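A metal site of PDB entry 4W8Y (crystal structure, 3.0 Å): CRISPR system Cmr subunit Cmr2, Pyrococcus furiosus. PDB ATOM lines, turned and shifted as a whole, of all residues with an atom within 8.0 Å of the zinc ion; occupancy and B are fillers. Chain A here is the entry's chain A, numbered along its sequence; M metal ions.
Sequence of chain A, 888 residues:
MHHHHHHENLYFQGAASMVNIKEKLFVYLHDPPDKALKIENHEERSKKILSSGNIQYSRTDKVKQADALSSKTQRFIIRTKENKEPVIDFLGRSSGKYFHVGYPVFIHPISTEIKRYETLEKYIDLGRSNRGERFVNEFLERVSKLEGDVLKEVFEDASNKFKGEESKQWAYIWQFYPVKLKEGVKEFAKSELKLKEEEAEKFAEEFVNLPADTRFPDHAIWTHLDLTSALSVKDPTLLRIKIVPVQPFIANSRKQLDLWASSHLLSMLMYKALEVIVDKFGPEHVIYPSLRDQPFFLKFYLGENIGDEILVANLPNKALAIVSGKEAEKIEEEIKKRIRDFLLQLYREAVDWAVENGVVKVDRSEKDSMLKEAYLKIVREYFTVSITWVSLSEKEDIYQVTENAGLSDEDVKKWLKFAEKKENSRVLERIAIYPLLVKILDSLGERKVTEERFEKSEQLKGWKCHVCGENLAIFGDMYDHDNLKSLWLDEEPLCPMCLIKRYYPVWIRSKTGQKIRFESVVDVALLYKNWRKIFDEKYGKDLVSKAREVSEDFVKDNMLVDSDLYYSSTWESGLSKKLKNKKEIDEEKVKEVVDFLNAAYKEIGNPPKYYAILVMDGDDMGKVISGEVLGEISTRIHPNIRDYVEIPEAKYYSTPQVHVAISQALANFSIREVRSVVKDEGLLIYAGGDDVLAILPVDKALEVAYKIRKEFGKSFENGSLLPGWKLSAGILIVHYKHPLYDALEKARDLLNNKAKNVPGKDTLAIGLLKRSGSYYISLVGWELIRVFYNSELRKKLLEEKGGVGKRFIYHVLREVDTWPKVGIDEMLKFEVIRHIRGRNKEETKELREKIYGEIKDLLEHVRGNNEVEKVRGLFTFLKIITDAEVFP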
ATOM      1  N   ASN A 252       4.383  -7.216  14.492  1.00  0.00           N
ATOM      2  CA  ASN A 252       4.423  -6.163  15.494  1.00  0.00           C
ATOM      3  C   ASN A 252       5.623  -6.327  16.430  1.00  0.00           C
ATOM      4  O   ASN A 252       5.510  -6.118  17.634  1.00  0.00           O
ATOM      5  CB  ASN A 252       3.126  -6.158  16.305  1.00  0.00           C
ATOM      6  CG  ASN A 252       2.773  -4.799  16.854  1.00  0.00           C
ATOM      7  OD1 ASN A 252       3.637  -3.922  16.978  1.00  0.00           O
ATOM      8  ND2 ASN A 252       1.498  -4.598  17.180  1.00  0.00           N
ATOM      9  N   TYR A 382      -6.264 -14.282  23.247  1.00  0.00           N
ATOM     10  CA  TYR A 382      -5.467 -13.641  22.192  1.00  0.00           C
ATOM     11  C   TYR A 382      -5.499 -14.433  20.889  1.00  0.00           C
ATOM     12  O   TYR A 382      -5.748 -13.866  19.829  1.00  0.00           O
ATOM     13  CB  TYR A 382      -4.012 -13.449  22.644  1.00  0.00           C
ATOM     14  CG  TYR A 382      -3.222 -12.554  21.715  1.00  0.00           C
ATOM     15  CD1 TYR A 382      -2.476 -13.090  20.683  1.00  0.00           C
ATOM     16  CD2 TYR A 382      -3.242 -11.169  21.871  1.00  0.00           C
ATOM     17  CE1 TYR A 382      -1.754 -12.275  19.823  1.00  0.00           C
ATOM     18  CE2 TYR A 382      -2.521 -10.344  21.012  1.00  0.00           C
ATOM     19  CZ  TYR A 382      -1.779 -10.902  19.984  1.00  0.00           C
ATOM     20  OH  TYR A 382      -1.062 -10.098  19.130  1.00  0.00           O
ATOM     21  N   LYS A 464      -0.993   0.897  28.111  1.00  0.00           N
ATOM     22  CA  LYS A 464      -0.675  -0.149  27.139  1.00  0.00           C
ATOM     23  C   LYS A 464       0.793  -0.588  27.198  1.00  0.00           C
ATOM     24  O   LYS A 464       1.656   0.160  27.659  1.00  0.00           O
ATOM     25  CB  LYS A 464      -1.031   0.323  25.727  1.00  0.00           C
ATOM     26  CG  LYS A 464      -2.508   0.627  25.545  1.00  0.00           C
ATOM     27  CD  LYS A 464      -3.371  -0.568  25.948  1.00  0.00           C
ATOM     28  CE  LYS A 464      -4.838  -0.205  26.081  1.00  0.00           C
ATOM     29  NZ  LYS A 464      -5.111   0.626  27.287  1.00  0.00           N
ATOM     30  N   CYS A 465       1.051  -1.797  26.710  1.00  0.00           N
ATOM     31  CA  CYS A 465       2.390  -2.356  26.663  1.00  0.00           C
ATOM     32  C   CYS A 465       3.359  -1.476  25.875  1.00  0.00           C
ATOM     33  O   CYS A 465       3.031  -0.986  24.806  1.00  0.00           O
ATOM     34  CB  CYS A 465       2.347  -3.756  26.040  1.00  0.00           C
ATOM     35  SG  CYS A 465       3.950  -4.466  25.601  1.00  0.00           S
ATOM     36  N   HIS A 466       4.545  -1.285  26.432  1.00  0.00           N
ATOM     37  CA  HIS A 466       5.559  -0.440  25.789  1.00  0.00           C
ATOM     38  C   HIS A 466       6.187  -1.108  24.578  1.00  0.00           C
ATOM     39  O   HIS A 466       6.836  -0.445  23.773  1.00  0.00           O
ATOM     40  CB  HIS A 466       6.654  -0.057  26.791  1.00  0.00           C
ATOM     41  CG  HIS A 466       6.294   1.089  27.676  1.00  0.00           C
ATOM     42  ND1 HIS A 466       7.236   1.904  28.260  1.00  0.00           N
ATOM     43  CD2 HIS A 466       5.082   1.564  28.073  1.00  0.00           C
ATOM     44  CE1 HIS A 466       6.629   2.832  28.971  1.00  0.00           C
ATOM     45  NE2 HIS A 466       5.324   2.652  28.881  1.00  0.00           N
ATOM     46  N   VAL A 467       6.015  -2.421  24.450  1.00  0.00           N
ATOM     47  CA  VAL A 467       6.600  -3.156  23.327  1.00  0.00           C
ATOM     48  C   VAL A 467       5.656  -3.227  22.125  1.00  0.00           C
ATOM     49  O   VAL A 467       6.074  -2.951  20.994  1.00  0.00           O
ATOM     50  CB  VAL A 467       6.990  -4.585  23.749  1.00  0.00           C
ATOM     51  CG1 VAL A 467       7.509  -5.378  22.555  1.00  0.00           C
ATOM     52  CG2 VAL A 467       8.009  -4.543  24.871  1.00  0.00           C
ATOM     53  N   CYS A 468       4.397  -3.576  22.353  1.00  0.00           N
ATOM     54  CA  CYS A 468       3.435  -3.669  21.254  1.00  0.00           C
ATOM     55  C   CYS A 468       2.591  -2.405  21.126  1.00  0.00           C
ATOM     56  O   CYS A 468       2.488  -1.829  20.056  1.00  0.00           O
ATOM     57  CB  CYS A 468       2.537  -4.894  21.420  1.00  0.00           C
ATOM     58  SG  CYS A 468       1.496  -4.891  22.892  1.00  0.00           S
ATOM     59  N   GLY A 469       1.988  -1.990  22.235  1.00  0.00           N
ATOM     60  CA  GLY A 469       1.173  -0.781  22.241  1.00  0.00           C
ATOM     61  C   GLY A 469      -0.267  -1.026  21.856  1.00  0.00           C
ATOM     62  O   GLY A 469      -1.017  -0.092  21.605  1.00  0.00           O
ATOM     63  N   GLU A 470      -0.668  -2.299  21.812  1.00  0.00           N
ATOM     64  CA  GLU A 470      -2.041  -2.667  21.472  1.00  0.00           C
ATOM     65  C   GLU A 470      -2.723  -3.464  22.589  1.00  0.00           C
ATOM     66  O   GLU A 470      -3.930  -3.690  22.542  1.00  0.00           O
ATOM     67  CB  GLU A 470      -2.079  -3.460  20.161  1.00  0.00           C
ATOM     68  CG  GLU A 470      -2.306  -2.608  18.926  1.00  0.00           C
ATOM     69  CD  GLU A 470      -1.013  -2.060  18.344  1.00  0.00           C
ATOM     70  OE1 GLU A 470       0.061  -2.506  18.792  1.00  0.00           O
ATOM     71  OE2 GLU A 470      -1.086  -1.194  17.444  1.00  0.00           O
ATOM     72  N   ASN A 471      -1.946  -3.890  23.577  1.00  0.00           N
ATOM     73  CA  ASN A 471      -2.484  -4.697  24.660  1.00  0.00           C
ATOM     74  C   ASN A 471      -2.232  -4.070  26.022  1.00  0.00           C
ATOM     75  O   ASN A 471      -1.217  -3.394  26.221  1.00  0.00           O
ATOM     76  CB  ASN A 471      -1.896  -6.101  24.628  1.00  0.00           C
ATOM     77  CG  ASN A 471      -2.473  -6.954  23.503  1.00  0.00           C
ATOM     78  OD1 ASN A 471      -3.603  -7.421  23.591  1.00  0.00           O
ATOM     79  ND2 ASN A 471      -1.682  -7.173  22.451  1.00  0.00           N
ATOM     80  N   LEU A 472      -3.153  -4.296  26.940  1.00  0.00           N
ATOM     81  CA  LEU A 472      -3.045  -3.801  28.308  1.00  0.00           C
ATOM     82  C   LEU A 472      -1.799  -4.346  29.010  1.00  0.00           C
ATOM     83  O   LEU A 472      -1.577  -5.552  29.040  1.00  0.00           O
ATOM     84  CB  LEU A 472      -4.286  -4.173  29.115  1.00  0.00           C
ATOM     85  CG  LEU A 472      -4.149  -4.063  30.639  1.00  0.00           C
ATOM     86  CD1 LEU A 472      -4.046  -2.614  31.074  1.00  0.00           C
ATOM     87  CD2 LEU A 472      -5.305  -4.766  31.330  1.00  0.00           C
ATOM     88  N   ALA A 473      -0.993  -3.443  29.566  1.00  0.00           N
ATOM     89  CA  ALA A 473       0.191  -3.869  30.294  1.00  0.00           C
ATOM     90  C   ALA A 473      -0.190  -4.382  31.677  1.00  0.00           C
ATOM     91  O   ALA A 473      -1.164  -3.928  32.273  1.00  0.00           O
ATOM     92  CB  ALA A 473       1.180  -2.720  30.403  1.00  0.00           C
ATOM     93  N   PRO A 493       6.993  -1.415  30.808  1.00  0.00           N
ATOM     94  CA  PRO A 493       5.828  -2.254  31.125  1.00  0.00           C
ATOM     95  C   PRO A 493       5.468  -3.218  30.008  1.00  0.00           C
ATOM     96  O   PRO A 493       5.507  -2.861  28.833  1.00  0.00           O
ATOM     97  CB  PRO A 493       4.713  -1.224  31.334  1.00  0.00           C
ATOM     98  CG  PRO A 493       5.404   0.027  31.726  1.00  0.00           C
ATOM     99  CD  PRO A 493       6.713   0.018  30.995  1.00  0.00           C
ATOM    100  N   LEU A 494       5.108  -4.445  30.382  1.00  0.00           N
ATOM    101  CA  LEU A 494       4.809  -5.500  29.413  1.00  0.00           C
ATOM    102  C   LEU A 494       3.382  -6.021  29.567  1.00  0.00           C
ATOM    103  O   LEU A 494       2.869  -6.160  30.672  1.00  0.00           O
ATOM    104  CB  LEU A 494       5.801  -6.657  29.584  1.00  0.00           C
ATOM    105  CG  LEU A 494       6.982  -6.745  28.629  1.00  0.00           C
ATOM    106  CD1 LEU A 494       7.692  -5.408  28.509  1.00  0.00           C
ATOM    107  CD2 LEU A 494       7.952  -7.817  29.099  1.00  0.00           C
ATOM    108  N   CYS A 495       2.745  -6.313  28.436  1.00  0.00           N
ATOM    109  CA  CYS A 495       1.458  -6.997  28.432  1.00  0.00           C
ATOM    110  C   CYS A 495       1.739  -8.491  28.626  1.00  0.00           C
ATOM    111  O   CYS A 495       2.882  -8.926  28.468  1.00  0.00           O
ATOM    112  CB  CYS A 495       0.702  -6.727  27.138  1.00  0.00           C
ATOM    113  SG  CYS A 495       1.404  -7.524  25.679  1.00  0.00           S
ATOM    114  N   PRO A 496       0.705  -9.276  28.978  1.00  0.00           N
ATOM    115  CA  PRO A 496       0.933 -10.708  29.158  1.00  0.00           C
ATOM    116  C   PRO A 496       1.573 -11.394  27.940  1.00  0.00           C
ATOM    117  O   PRO A 496       2.533 -12.136  28.093  1.00  0.00           O
ATOM    118  CB  PRO A 496      -0.476 -11.243  29.413  1.00  0.00           C
ATOM    119  CG  PRO A 496      -1.179 -10.115  30.068  1.00  0.00           C
ATOM    120  CD  PRO A 496      -0.650  -8.873  29.401  1.00  0.00           C
ATOM    121  N   MET A 497       1.041 -11.118  26.752  1.00  0.00           N
ATOM    122  CA  MET A 497       1.528 -11.763  25.533  1.00  0.00           C
ATOM    123  C   MET A 497       2.986 -11.419  25.243  1.00  0.00           C
ATOM    124  O   MET A 497       3.757 -12.264  24.804  1.00  0.00           O
ATOM    125  CB  MET A 497       0.649 -11.382  24.350  1.00  0.00           C
ATOM    126  CG  MET A 497      -0.802 -11.804  24.490  1.00  0.00           C
ATOM    127  SD  MET A 497      -0.979 -13.588  24.613  1.00  0.00           S
ATOM    128  CE  MET A 497       0.073 -14.131  23.273  1.00  0.00           C
ATOM    129  N   CYS A 498       3.356 -10.169  25.489  1.00  0.00           N
ATOM    130  CA  CYS A 498       4.725  -9.716  25.271  1.00  0.00           C
ATOM    131  C   CYS A 498       5.665 -10.260  26.344  1.00  0.00           C
ATOM    132  O   CYS A 498       6.848 -10.455  26.087  1.00  0.00           O
ATOM    133  CB  CYS A 498       4.790  -8.196  25.214  1.00  0.00           C
ATOM    134  SG  CYS A 498       4.256  -7.501  23.633  1.00  0.00           S
ATOM    135  N   LEU A 499       5.141 -10.490  27.539  1.00  0.00           N
ATOM    136  CA  LEU A 499       5.941 -11.091  28.597  1.00  0.00           C
ATOM    137  C   LEU A 499       6.255 -12.545  28.248  1.00  0.00           C
ATOM    138  O   LEU A 499       7.389 -13.005  28.386  1.00  0.00           O
ATOM    139  CB  LEU A 499       5.223 -11.013  29.943  1.00  0.00           C
ATOM    140  CG  LEU A 499       5.942 -11.749  31.085  1.00  0.00           C
ATOM    141  CD1 LEU A 499       7.294 -11.126  31.383  1.00  0.00           C
ATOM    142  CD2 LEU A 499       5.079 -11.795  32.336  1.00  0.00           C
ATOM    143  N   LYS A 501       6.285 -13.601  25.292  1.00  0.00           N
ATOM    144  CA  LYS A 501       7.134 -13.462  24.120  1.00  0.00           C
ATOM    145  C   LYS A 501       8.590 -13.236  24.519  1.00  0.00           C
ATOM    146  O   LYS A 501       9.515 -13.650  23.807  1.00  0.00           O
ATOM    147  CB  LYS A 501       6.629 -12.316  23.240  1.00  0.00           C
ATOM    148  CG  LYS A 501       6.970 -12.469  21.783  1.00  0.00           C
ATOM    149  CD  LYS A 501       5.948 -11.754  20.911  1.00  0.00           C
ATOM    150  CE  LYS A 501       6.155 -10.249  20.899  1.00  0.00           C
ATOM    151  NZ  LYS A 501       5.287  -9.594  19.888  1.00  0.00           N
HETATM  152 ZN    ZN M   1       2.696  -6.036  24.464  1.00  0.00          ZN
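The backbone NH (N) of Cys 465 lies within hydrogen-bond range of the backbone carbonyl oxygen (O) of Asn 471. The backbone NH of Asn 471 sits close to the side-chain sulfur of Cys 468 (3.6 Å). The backbone NH of Val 467 sits close to the side-chain sulfur of Cys 465, 3.1 Å away. The backbone NH (N) of Glu 470 sits close to the side-chain sulfur (SG) of Cys 468. N of Met 497 lies close to SG of Cys 495, 3.8 Å away.
Along chain A the residues within 4 Å of the zinc ion span positions 465 to 498. The nearest printed residue that does not touch the zinc ion is Val 467 (4.6 Å).
The zinc ion is bound by SG of Cys 468 (2.3 Å), SG of Cys 498 (2.3 Å), SG of Cys 465 (2.3 Å) and SG of Cys 495 (2.3 Å).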
